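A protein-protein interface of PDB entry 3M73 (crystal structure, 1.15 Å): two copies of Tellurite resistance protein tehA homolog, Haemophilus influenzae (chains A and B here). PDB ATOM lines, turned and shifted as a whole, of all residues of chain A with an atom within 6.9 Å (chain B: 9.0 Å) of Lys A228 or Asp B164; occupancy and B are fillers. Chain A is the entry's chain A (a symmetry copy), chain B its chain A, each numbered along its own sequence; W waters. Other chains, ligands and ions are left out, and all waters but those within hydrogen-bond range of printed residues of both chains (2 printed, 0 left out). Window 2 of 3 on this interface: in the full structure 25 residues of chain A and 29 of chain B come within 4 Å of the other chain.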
ATOM      1  N   VAL A 212      -9.836 -11.699  15.332  1.00  0.00           N
ATOM      2  CA  VAL A 212      -9.009 -12.314  14.323  1.00  0.00           C
ATOM      3  C   VAL A 212      -7.567 -12.430  14.764  1.00  0.00           C
ATOM      4  O   VAL A 212      -6.903 -13.416  14.410  1.00  0.00           O
ATOM      5  CB  VAL A 212      -9.157 -11.632  12.945  1.00  0.00           C
ATOM      6  CG1 VAL A 212      -8.463 -10.288  12.868  1.00  0.00           C
ATOM      7  CG2 VAL A 212      -8.664 -12.546  11.806  1.00  0.00           C
ATOM      8  N   VAL A 223      -4.406 -17.761   7.295  1.00  0.00           N
ATOM      9  CA  VAL A 223      -5.410 -16.777   6.911  1.00  0.00           C
ATOM     10  C   VAL A 223      -6.473 -17.409   6.050  1.00  0.00           C
ATOM     11  O   VAL A 223      -6.310 -17.559   4.840  1.00  0.00           O
ATOM     12  CB  VAL A 223      -4.767 -15.596   6.176  1.00  0.00           C
ATOM     13  CG1 VAL A 223      -5.832 -14.616   5.801  1.00  0.00           C
ATOM     14  CG2 VAL A 223      -3.712 -14.945   7.052  1.00  0.00           C
ATOM     15  N   ASP A 224      -7.547 -17.815   6.663  1.00  0.00           N
ATOM     16  CA  ASP A 224      -8.588 -18.596   6.059  1.00  0.00           C
ATOM     17  C   ASP A 224      -9.850 -17.774   5.879  1.00  0.00           C
ATOM     18  O   ASP A 224      -9.875 -16.570   6.033  1.00  0.00           O
ATOM     19  CB  ASP A 224      -8.807 -19.850   6.903  1.00  0.00           C
ATOM     20  CG  ASP A 224      -9.289 -19.549   8.286  1.00  0.00           C
ATOM     21  OD1 ASP A 224      -9.562 -18.393   8.624  1.00  0.00           O
ATOM     22  OD2 ASP A 224      -9.426 -20.533   9.067  1.00  0.00           O
ATOM     23  N   THR A 225     -10.949 -18.443   5.530  1.00  0.00           N
ATOM     24  CA  THR A 225     -12.197 -17.740   5.262  1.00  0.00           C
ATOM     25  C   THR A 225     -12.690 -16.993   6.502  1.00  0.00           C
ATOM     26  O   THR A 225     -13.098 -15.832   6.401  1.00  0.00           O
ATOM     27  CB  THR A 225     -13.248 -18.706   4.750  1.00  0.00           C
ATOM     28  OG1 THR A 225     -12.796 -19.140   3.471  1.00  0.00           O
ATOM     29  CG2 THR A 225     -14.601 -18.047   4.638  1.00  0.00           C
ATOM     30  N   LEU A 226     -12.655 -17.625   7.680  1.00  0.00           N
ATOM     31  CA  LEU A 226     -13.065 -16.934   8.888  1.00  0.00           C
ATOM     32  C   LEU A 226     -12.240 -15.664   9.102  1.00  0.00           C
ATOM     33  O   LEU A 226     -12.785 -14.622   9.436  1.00  0.00           O
ATOM     34  CB  LEU A 226     -12.964 -17.839  10.103  1.00  0.00           C
ATOM     35  CG  LEU A 226     -13.290 -17.154  11.430  1.00  0.00           C
ATOM     36  CD1 LEU A 226     -14.696 -16.544  11.464  1.00  0.00           C
ATOM     37  CD2 LEU A 226     -13.088 -18.120  12.560  1.00  0.00           C
ATOM     38  N   ALA A 227     -10.930 -15.757   8.934  1.00  0.00           N
ATOM     39  CA  ALA A 227     -10.079 -14.587   9.157  1.00  0.00           C
ATOM     40  C   ALA A 227     -10.481 -13.444   8.225  1.00  0.00           C
ATOM     41  O   ALA A 227     -10.533 -12.296   8.636  1.00  0.00           O
ATOM     42  CB  ALA A 227      -8.635 -14.942   8.976  1.00  0.00           C
ATOM     43  N   LYS A 228     -10.714 -13.758   6.944  1.00  0.00           N
ATOM     44  CA  LYS A 228     -11.083 -12.732   5.987  1.00  0.00           C
ATOM     45  C   LYS A 228     -12.438 -12.113   6.334  1.00  0.00           C
ATOM     46  O   LYS A 228     -12.626 -10.889   6.232  1.00  0.00           O
ATOM     47  CB  LYS A 228     -11.108 -13.318   4.578  1.00  0.00           C
ATOM     48  CG  LYS A 228      -9.739 -13.795   4.094  1.00  0.00           C
ATOM     49  CD  LYS A 228      -9.840 -14.584   2.771  1.00  0.00           C
ATOM     50  CE  LYS A 228      -8.592 -15.359   2.458  1.00  0.00           C
ATOM     51  NZ  LYS A 228      -8.773 -16.212   1.257  1.00  0.00           N
ATOM     52  N   ILE A 229     -13.381 -12.942   6.751  1.00  0.00           N
ATOM     53  CA  ILE A 229     -14.702 -12.475   7.173  1.00  0.00           C
ATOM     54  C   ILE A 229     -14.604 -11.469   8.315  1.00  0.00           C
ATOM     55  O   ILE A 229     -15.236 -10.421   8.321  1.00  0.00           O
ATOM     56  CB  ILE A 229     -15.584 -13.687   7.556  1.00  0.00           C
ATOM     57  CG1 ILE A 229     -16.092 -14.352   6.293  1.00  0.00           C
ATOM     58  CG2 ILE A 229     -16.708 -13.332   8.540  1.00  0.00           C
ATOM     59  CD1 ILE A 229     -16.791 -15.673   6.502  1.00  0.00           C
ATOM     60  N   LEU A 230     -13.778 -11.796   9.315  1.00  0.00           N
ATOM     61  CA  LEU A 230     -13.599 -10.934  10.447  1.00  0.00           C
ATOM     62  C   LEU A 230     -12.972  -9.613  10.058  1.00  0.00           C
ATOM     63  O   LEU A 230     -13.382  -8.558  10.529  1.00  0.00           O
ATOM     64  CB  LEU A 230     -12.743 -11.644  11.506  1.00  0.00           C
ATOM     65  CG  LEU A 230     -13.414 -12.843  12.199  1.00  0.00           C
ATOM     66  CD1 LEU A 230     -12.414 -13.671  12.945  1.00  0.00           C
ATOM     67  CD2 LEU A 230     -14.531 -12.391  13.110  1.00  0.00           C
ATOM     68  N   TRP A 231     -11.956  -9.673   9.188  1.00  0.00           N
ATOM     69  CA  TRP A 231     -11.355  -8.439   8.735  1.00  0.00           C
ATOM     70  C   TRP A 231     -12.382  -7.562   8.030  1.00  0.00           C
ATOM     71  O   TRP A 231     -12.366  -6.344   8.148  1.00  0.00           O
ATOM     72  CB  TRP A 231     -10.161  -8.716   7.811  1.00  0.00           C
ATOM     73  CG  TRP A 231      -8.852  -8.290   8.352  1.00  0.00           C
ATOM     74  CD1 TRP A 231      -8.518  -8.200   9.655  1.00  0.00           C
ATOM     75  CD2 TRP A 231      -7.715  -7.889   7.611  1.00  0.00           C
ATOM     76  NE1 TRP A 231      -7.237  -7.761   9.795  1.00  0.00           N
ATOM     77  CE2 TRP A 231      -6.726  -7.549   8.549  1.00  0.00           C
ATOM     78  CE3 TRP A 231      -7.439  -7.757   6.258  1.00  0.00           C
ATOM     79  CZ2 TRP A 231      -5.467  -7.088   8.185  1.00  0.00           C
ATOM     80  CZ3 TRP A 231      -6.136  -7.302   5.897  1.00  0.00           C
ATOM     81  CH2 TRP A 231      -5.211  -6.972   6.874  1.00  0.00           C
ATOM     82  N   GLY A 232     -13.273  -8.161   7.243  1.00  0.00           N
ATOM     83  CA  GLY A 232     -14.235  -7.356   6.520  1.00  0.00           C
ATOM     84  C   GLY A 232     -15.136  -6.573   7.445  1.00  0.00           C
ATOM     85  O   GLY A 232     -15.351  -5.385   7.262  1.00  0.00           O
ATOM     86  N   TYR A 233     -15.696  -7.239   8.457  1.00  0.00           N
ATOM     87  CA  TYR A 233     -16.518  -6.511   9.408  1.00  0.00           C
ATOM     88  C   TYR A 233     -15.682  -5.500  10.201  1.00  0.00           C
ATOM     89  O   TYR A 233     -16.133  -4.398  10.473  1.00  0.00           O
ATOM     90  CB  TYR A 233     -17.244  -7.461  10.346  1.00  0.00           C
ATOM     91  CG  TYR A 233     -18.284  -6.794  11.203  1.00  0.00           C
ATOM     92  CD1 TYR A 233     -19.504  -6.455  10.674  1.00  0.00           C
ATOM     93  CD2 TYR A 233     -18.067  -6.496  12.537  1.00  0.00           C
ATOM     94  CE1 TYR A 233     -20.471  -5.858  11.440  1.00  0.00           C
ATOM     95  CE2 TYR A 233     -19.040  -5.880  13.314  1.00  0.00           C
ATOM     96  CZ  TYR A 233     -20.251  -5.584  12.762  1.00  0.00           C
ATOM     97  OH  TYR A 233     -21.282  -5.014  13.491  1.00  0.00           O
ATOM     98  N   GLY A 234     -14.452  -5.876  10.527  1.00  0.00           N
ATOM     99  CA  GLY A 234     -13.576  -4.942  11.230  1.00  0.00           C
ATOM    100  C   GLY A 234     -13.362  -3.656  10.456  1.00  0.00           C
ATOM    101  O   GLY A 234     -13.424  -2.564  11.053  1.00  0.00           O
ATOM    102  N   PHE A 274      -1.863 -11.420   7.657  1.00  0.00           N
ATOM    103  CA  PHE A 274      -2.356 -11.312   6.297  1.00  0.00           C
ATOM    104  C   PHE A 274      -1.175 -11.107   5.338  1.00  0.00           C
ATOM    105  O   PHE A 274      -1.102 -11.747   4.290  1.00  0.00           O
ATOM    106  CB  PHE A 274      -3.401 -10.195   6.179  1.00  0.00           C
ATOM    107  CG  PHE A 274      -4.786 -10.636   6.587  1.00  0.00           C
ATOM    108  CD1 PHE A 274      -5.123 -10.794   7.910  1.00  0.00           C
ATOM    109  CD2 PHE A 274      -5.751 -10.865   5.640  1.00  0.00           C
ATOM    110  CE1 PHE A 274      -6.397 -11.198   8.285  1.00  0.00           C
ATOM    111  CE2 PHE A 274      -7.032 -11.240   6.004  1.00  0.00           C
ATOM    112  CZ  PHE A 274      -7.342 -11.410   7.329  1.00  0.00           C
ATOM    113  N   ASN A 278       0.304 -13.660   2.291  1.00  0.00           N
ATOM    114  CA  ASN A 278       0.068 -13.121   0.969  1.00  0.00           C
ATOM    115  C   ASN A 278      -1.418 -12.980   0.663  1.00  0.00           C
ATOM    116  O   ASN A 278      -1.878 -13.343  -0.428  1.00  0.00           O
ATOM    117  CB  ASN A 278       0.766 -13.941  -0.120  1.00  0.00           C
ATOM    118  CG  ASN A 278       0.797 -13.203  -1.454  1.00  0.00           C
ATOM    119  OD1 ASN A 278       0.723 -11.984  -1.502  1.00  0.00           O
ATOM    120  ND2 ASN A 278       0.928 -13.955  -2.546  1.00  0.00           N
ATOM    121  N   VAL A 279      -2.156 -12.418   1.612  1.00  0.00           N
ATOM    122  CA  VAL A 279      -3.566 -12.089   1.442  1.00  0.00           C
ATOM    123  C   VAL A 279      -3.711 -10.604   1.637  1.00  0.00           C
ATOM    124  O   VAL A 279      -3.388 -10.072   2.701  1.00  0.00           O
ATOM    125  CB  VAL A 279      -4.468 -12.838   2.464  1.00  0.00           C
ATOM    126  CG1 VAL A 279      -5.909 -12.437   2.302  1.00  0.00           C
ATOM    127  CG2 VAL A 279      -4.332 -14.340   2.273  1.00  0.00           C
ATOM    128  N   LEU A 280      -4.200  -9.930   0.627  1.00  0.00           N
ATOM    129  CA  LEU A 280      -4.467  -8.502   0.719  1.00  0.00           C
ATOM    130  C   LEU A 280      -3.279  -7.738   1.274  1.00  0.00           C
ATOM    131  O   LEU A 280      -3.380  -6.971   2.235  1.00  0.00           O
ATOM    132  CB  LEU A 280      -5.703  -8.276   1.572  1.00  0.00           C
ATOM    133  CG  LEU A 280      -6.985  -8.888   0.986  1.00  0.00           C
ATOM    134  CD1 LEU A 280      -8.097  -8.865   2.022  1.00  0.00           C
ATOM    135  CD2 LEU A 280      -7.419  -8.140  -0.273  1.00  0.00           C
ATOM    136  N   SER B 153     -21.779  -6.545  -3.352  1.00  0.00           N
ATOM    137  CA  SER B 153     -20.400  -6.229  -3.638  1.00  0.00           C
ATOM    138  C   SER B 153     -19.526  -7.473  -3.596  1.00  0.00           C
ATOM    139  O   SER B 153     -18.634  -7.664  -4.414  1.00  0.00           O
ATOM    140  CB  SER B 153     -19.871  -5.189  -2.672  1.00  0.00           C
ATOM    141  OG  SER B 153     -20.367  -3.883  -2.946  1.00  0.00           O
ATOM    142  N   ALA B 154     -19.742  -8.336  -2.608  1.00  0.00           N
ATOM    143  CA  ALA B 154     -18.942  -9.547  -2.475  1.00  0.00           C
ATOM    144  C   ALA B 154     -18.991 -10.397  -3.723  1.00  0.00           C
ATOM    145  O   ALA B 154     -17.950 -10.811  -4.243  1.00  0.00           O
ATOM    146  CB  ALA B 154     -19.405 -10.337  -1.267  1.00  0.00           C
ATOM    147  N   LEU B 157     -17.542  -8.460  -6.902  1.00  0.00           N
ATOM    148  CA  LEU B 157     -16.096  -8.370  -6.895  1.00  0.00           C
ATOM    149  C   LEU B 157     -15.501  -9.730  -7.194  1.00  0.00           C
ATOM    150  O   LEU B 157     -14.494  -9.825  -7.917  1.00  0.00           O
ATOM    151  CB  LEU B 157     -15.599  -7.783  -5.573  1.00  0.00           C
ATOM    152  CG  LEU B 157     -15.867  -6.297  -5.408  1.00  0.00           C
ATOM    153  CD1 LEU B 157     -15.535  -5.877  -4.003  1.00  0.00           C
ATOM    154  CD2 LEU B 157     -15.156  -5.408  -6.385  1.00  0.00           C
ATOM    155  N   ALA B 158     -16.088 -10.809  -6.673  1.00  0.00           N
ATOM    156  CA  ALA B 158     -15.619 -12.142  -7.021  1.00  0.00           C
ATOM    157  C   ALA B 158     -15.713 -12.418  -8.519  1.00  0.00           C
ATOM    158  O   ALA B 158     -14.804 -12.995  -9.115  1.00  0.00           O
ATOM    159  CB  ALA B 158     -16.334 -13.202  -6.223  1.00  0.00           C
ATOM    160  N   GLY B 161     -12.848 -11.255 -10.274  1.00  0.00           N
ATOM    161  CA  GLY B 161     -11.607 -11.904  -9.876  1.00  0.00           C
ATOM    162  C   GLY B 161     -11.008 -11.441  -8.583  1.00  0.00           C
ATOM    163  O   GLY B 161      -9.901 -11.846  -8.253  1.00  0.00           O
ATOM    164  N   TYR B 162     -11.724 -10.598  -7.843  1.00  0.00           N
ATOM    165  CA  TYR B 162     -11.208 -10.067  -6.590  1.00  0.00           C
ATOM    166  C   TYR B 162     -11.798 -10.831  -5.422  1.00  0.00           C
ATOM    167  O   TYR B 162     -12.548 -10.286  -4.601  1.00  0.00           O
ATOM    168  CB  TYR B 162     -11.506  -8.571  -6.448  1.00  0.00           C
ATOM    169  CG  TYR B 162     -10.882  -7.721  -7.506  1.00  0.00           C
ATOM    170  CD1 TYR B 162      -9.571  -7.294  -7.376  1.00  0.00           C
ATOM    171  CD2 TYR B 162     -11.602  -7.295  -8.594  1.00  0.00           C
ATOM    172  CE1 TYR B 162      -8.984  -6.484  -8.347  1.00  0.00           C
ATOM    173  CE2 TYR B 162     -11.012  -6.510  -9.604  1.00  0.00           C
ATOM    174  CZ  TYR B 162      -9.710  -6.124  -9.455  1.00  0.00           C
ATOM    175  OH  TYR B 162      -9.087  -5.336 -10.414  1.00  0.00           O
ATOM    176  N   HIS B 163     -11.456 -12.101  -5.318  1.00  0.00           N
ATOM    177  CA  HIS B 163     -12.114 -12.960  -4.330  1.00  0.00           C
ATOM    178  C   HIS B 163     -11.837 -12.528  -2.901  1.00  0.00           C
ATOM    179  O   HIS B 163     -12.760 -12.554  -2.082  1.00  0.00           O
ATOM    180  CB  HIS B 163     -11.724 -14.410  -4.516  1.00  0.00           C
ATOM    181  CG  HIS B 163     -12.138 -14.969  -5.835  1.00  0.00           C
ATOM    182  ND1 HIS B 163     -11.506 -14.622  -7.003  1.00  0.00           N
ATOM    183  CD2 HIS B 163     -13.168 -15.779  -6.187  1.00  0.00           C
ATOM    184  CE1 HIS B 163     -12.090 -15.245  -8.008  1.00  0.00           C
ATOM    185  NE2 HIS B 163     -13.102 -15.948  -7.551  1.00  0.00           N
ATOM    186  N   ASP B 164     -10.601 -12.182  -2.571  1.00  0.00           N
ATOM    187  CA  ASP B 164     -10.297 -11.824  -1.194  1.00  0.00           C
ATOM    188  C   ASP B 164     -10.961 -10.521  -0.800  1.00  0.00           C
ATOM    189  O   ASP B 164     -11.501 -10.437   0.315  1.00  0.00           O
ATOM    190  CB  ASP B 164      -8.796 -11.805  -0.938  1.00  0.00           C
ATOM    191  CG  ASP B 164      -8.190 -13.173  -0.937  1.00  0.00           C
ATOM    192  OD1 ASP B 164      -8.928 -14.155  -0.690  1.00  0.00           O
ATOM    193  OD2 ASP B 164      -6.975 -13.259  -1.183  1.00  0.00           O
ATOM    194  N   LEU B 165     -10.987  -9.518  -1.678  1.00  0.00           N
ATOM    195  CA  LEU B 165     -11.757  -8.329  -1.405  1.00  0.00           C
ATOM    196  C   LEU B 165     -13.231  -8.682  -1.247  1.00  0.00           C
ATOM    197  O   LEU B 165     -13.962  -8.151  -0.393  1.00  0.00           O
ATOM    198  CB  LEU B 165     -11.577  -7.334  -2.535  1.00  0.00           C
ATOM    199  CG  LEU B 165     -10.479  -6.304  -2.552  1.00  0.00           C
ATOM    200  CD1 LEU B 165     -10.913  -5.286  -3.605  1.00  0.00           C
ATOM    201  CD2 LEU B 165     -10.302  -5.666  -1.183  1.00  0.00           C
ATOM    202  N   GLY B 166     -13.701  -9.596  -2.085  1.00  0.00           N
ATOM    203  CA  GLY B 166     -15.060 -10.071  -1.960  1.00  0.00           C
ATOM    204  C   GLY B 166     -15.347 -10.667  -0.585  1.00  0.00           C
ATOM    205  O   GLY B 166     -16.418 -10.425  -0.024  1.00  0.00           O
ATOM    206  N   TYR B 167     -14.422 -11.454  -0.048  1.00  0.00           N
ATOM    207  CA  TYR B 167     -14.619 -11.997   1.285  1.00  0.00           C
ATOM    208  C   TYR B 167     -14.736 -10.922   2.350  1.00  0.00           C
ATOM    209  O   TYR B 167     -15.465 -11.098   3.314  1.00  0.00           O
ATOM    210  CB  TYR B 167     -13.513 -12.982   1.669  1.00  0.00           C
ATOM    211  CG  TYR B 167     -13.712 -14.403   1.212  1.00  0.00           C
ATOM    212  CD1 TYR B 167     -12.828 -15.010   0.382  1.00  0.00           C
ATOM    213  CD2 TYR B 167     -14.825 -15.144   1.611  1.00  0.00           C
ATOM    214  CE1 TYR B 167     -12.991 -16.342  -0.046  1.00  0.00           C
ATOM    215  CE2 TYR B 167     -14.988 -16.467   1.213  1.00  0.00           C
ATOM    216  CZ  TYR B 167     -14.078 -17.039   0.366  1.00  0.00           C
ATOM    217  OH  TYR B 167     -14.250 -18.361  -0.044  1.00  0.00           O
ATOM    218  N   LEU B 168     -14.046  -9.797   2.189  1.00  0.00           N
ATOM    219  CA  LEU B 168     -14.186  -8.708   3.158  1.00  0.00           C
ATOM    220  C   LEU B 168     -15.619  -8.187   3.123  1.00  0.00           C
ATOM    221  O   LEU B 168     -16.239  -8.024   4.186  1.00  0.00           O
ATOM    222  CB  LEU B 168     -13.242  -7.552   2.851  1.00  0.00           C
ATOM    223  CG  LEU B 168     -11.754  -7.773   2.855  1.00  0.00           C
ATOM    224  CD1 LEU B 168     -10.990  -6.501   2.591  1.00  0.00           C
ATOM    225  CD2 LEU B 168     -11.426  -8.257   4.170  1.00  0.00           C
ATOM    226  N   PHE B 169     -16.146  -7.881   1.934  1.00  0.00           N
ATOM    227  CA  PHE B 169     -17.521  -7.433   1.871  1.00  0.00           C
ATOM    228  C   PHE B 169     -18.499  -8.497   2.369  1.00  0.00           C
ATOM    229  O   PHE B 169     -19.497  -8.183   3.003  1.00  0.00           O
ATOM    230  CB  PHE B 169     -17.868  -6.997   0.449  1.00  0.00           C
ATOM    231  CG  PHE B 169     -17.303  -5.632   0.105  1.00  0.00           C
ATOM    232  CD1 PHE B 169     -18.000  -4.479   0.453  1.00  0.00           C
ATOM    233  CD2 PHE B 169     -16.078  -5.485  -0.526  1.00  0.00           C
ATOM    234  CE1 PHE B 169     -17.488  -3.223   0.172  1.00  0.00           C
ATOM    235  CE2 PHE B 169     -15.577  -4.206  -0.800  1.00  0.00           C
ATOM    236  CZ  PHE B 169     -16.290  -3.109  -0.446  1.00  0.00           C
ATOM    237  N   PHE B 170     -18.215  -9.762   2.075  1.00  0.00           N
ATOM    238  CA  PHE B 170     -19.042 -10.868   2.542  1.00  0.00           C
ATOM    239  C   PHE B 170     -19.101 -10.878   4.057  1.00  0.00           C
ATOM    240  O   PHE B 170     -20.189 -11.003   4.632  1.00  0.00           O
ATOM    241  CB  PHE B 170     -18.482 -12.201   2.013  1.00  0.00           C
ATOM    242  CG  PHE B 170     -19.269 -13.370   2.489  1.00  0.00           C
ATOM    243  CD1 PHE B 170     -20.502 -13.674   1.961  1.00  0.00           C
ATOM    244  CD2 PHE B 170     -18.841 -14.106   3.567  1.00  0.00           C
ATOM    245  CE1 PHE B 170     -21.266 -14.688   2.478  1.00  0.00           C
ATOM    246  CE2 PHE B 170     -19.606 -15.152   4.080  1.00  0.00           C
ATOM    247  CZ  PHE B 170     -20.824 -15.418   3.536  1.00  0.00           C
ATOM    248  N   GLY B 171     -17.961 -10.775   4.711  1.00  0.00           N
ATOM    249  CA  GLY B 171     -17.947 -10.768   6.150  1.00  0.00           C
ATOM    250  C   GLY B 171     -18.659  -9.585   6.739  1.00  0.00           C
ATOM    251  O   GLY B 171     -19.343  -9.704   7.774  1.00  0.00           O
ATOM    252  N   ALA B 172     -18.479  -8.414   6.142  1.00  0.00           N
ATOM    253  CA  ALA B 172     -19.196  -7.250   6.587  1.00  0.00           C
ATOM    254  C   ALA B 172     -20.699  -7.511   6.559  1.00  0.00           C
ATOM    255  O   ALA B 172     -21.411  -7.200   7.509  1.00  0.00           O
ATOM    256  CB  ALA B 172     -18.811  -6.038   5.745  1.00  0.00           C
ATOM    257  N   ILE B 175     -21.807 -10.583   9.213  1.00  0.00           N
ATOM    258  CA  ILE B 175     -21.811 -10.193  10.602  1.00  0.00           C
ATOM    259  C   ILE B 175     -22.828  -9.069  10.829  1.00  0.00           C
ATOM    260  O   ILE B 175     -23.531  -9.083  11.836  1.00  0.00           O
ATOM    261  CB  ILE B 175     -20.381  -9.915  11.100  1.00  0.00           C
ATOM    262  CG1 ILE B 175     -19.566 -11.226  11.025  1.00  0.00           C
ATOM    263  CG2 ILE B 175     -20.410  -9.389  12.528  1.00  0.00           C
ATOM    264  CD1 ILE B 175     -18.106 -11.081  11.330  1.00  0.00           C
ATOM    265  N   ILE B 218     -18.219 -16.602  -4.356  1.00  0.00           N
ATOM    266  CA  ILE B 218     -16.820 -16.429  -4.055  1.00  0.00           C
ATOM    267  C   ILE B 218     -16.085 -17.772  -4.064  1.00  0.00           C
ATOM    268  O   ILE B 218     -14.939 -17.870  -4.517  1.00  0.00           O
ATOM    269  CB  ILE B 218     -16.621 -15.725  -2.723  1.00  0.00           C
ATOM    270  CG1 ILE B 218     -17.311 -14.371  -2.669  1.00  0.00           C
ATOM    271  CG2 ILE B 218     -15.161 -15.591  -2.392  1.00  0.00           C
ATOM    272  CD1 ILE B 218     -17.477 -13.886  -1.259  1.00  0.00           C
ATOM    273  N   HIS B 220     -16.665 -20.559  -5.632  1.00  0.00           N
ATOM    274  CA  HIS B 220     -16.793 -21.397  -6.861  1.00  0.00           C
ATOM    275  C   HIS B 220     -17.839 -22.506  -6.726  1.00  0.00           C
ATOM    276  O   HIS B 220     -17.659 -23.622  -7.241  1.00  0.00           O
ATOM    277  CB  HIS B 220     -15.442 -22.027  -7.290  1.00  0.00           C
ATOM    278  CG  HIS B 220     -14.284 -21.078  -7.228  1.00  0.00           C
ATOM    279  ND1 HIS B 220     -13.912 -20.285  -8.294  1.00  0.00           N
ATOM    280  CD2 HIS B 220     -13.424 -20.786  -6.222  1.00  0.00           C
ATOM    281  CE1 HIS B 220     -12.877 -19.541  -7.942  1.00  0.00           C
ATOM    282  NE2 HIS B 220     -12.564 -19.822  -6.689  1.00  0.00           N
HETATM  283  O   HOH W   1      -5.200 -11.304  -1.734  1.00  0.00           O
HETATM  284  O   HOH W   2     -14.678 -20.433   2.011  1.00  0.00           O
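No position is printed for both chains.
The backbone NH (N) of Val A279 is in hydrogen-bond range of the backbone carbonyl oxygen (O) of Phe A274 (3.0 Å).
Of chain B, only Asp B164 (2.8 Å), Tyr B167 (3.8 Å) and Leu B168 (3.6 Å) come within 4 Å of Lys A228. Of chain A, only Lys A228 (2.8 Å), Val A279 (3.7 Å) and Leu A280 (3.9 Å) come within 4 Å of Asp B164. No residue of chain B comes within 4 Å of Ala A227. Of the printed residues of chain A, Leu B168 touches Lys A228, Trp A231, Gly A232 and Leu A280. Of the printed residues of chain B, Gly A232 touches Leu B168 (3.1 Å) and Ala B172 (3.8 Å). The nearest residue of chain B that does not touch Lys A228 is Gly B171 (5.3 Å). The nearest residue of chain A that does not touch Asp B164 is Asn A278 (5.2 Å).
Water W1 lies within hydrogen-bond range of OD2 of Asp B164 (2.7 Å) and N of Leu A280 (2.9 Å). Water W2 bridges the side-chain hydroxyl of Thr A225 (2.7 Å) and the side-chain hydroxyl of Tyr B167 (2.9 Å).
Of the 19 printed residues of chain B, 8 touch a printed residue of chain A. Printed residues of chain B that touch a printed residue of chain A: Asp B164, Leu B165, Tyr B167, Leu B168, Phe B170, Gly B171, Ala B172 and Ile B175. Hydrophobic or aromatic side chains of chain B within 4 Å of the printed part of chain A: Leu B165, Tyr B167, Leu B168, Phe B170, Ala B172 and Ile B175. Printed residues of chain A that touch a printed residue of chain B: Thr A225, Lys A228, Ile A229, Trp A231, Gly A232, Tyr A233, Val A279 and Leu A280. Among the printed residues, 16 pairs touch across the chains. Among the printed residues, Asp or Glu carboxylates within 4 Å of a Lys or Arg side-chain nitrogen of the other chain: Lys A228 with Asp B164 (2.8 Å).
CB of Tyr B167 touches CB of Lys A228 (3.8 Å). O of Lys A228 touches CD2 of Leu B168, at 3.6 Å. O of Ile A229 touches CA of Gly B171, at 3.5 Å. CG2 of Ile A229 touches CD1 of Ile B175, 3.8 Å away. Trp A231 touches Leu B168. O of Gly A232 touches CB of Ala B172 (3.8 Å). CD1 of Tyr A233 touches O of Ala B172 (3.8 Å). CD1 of Tyr A233 touches CG2 of Ile B175, 3.6 Å away. OD2 of Asp B164 touches CG1 of Val A279 (3.7 Å). CG of Leu A280 touches CB of Asp B164 (3.9 Å).
The side-chain carboxylate (OD1) of Asp B164 is in salt-bridge range of the side-chain amino group (NZ) of Lys A228.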
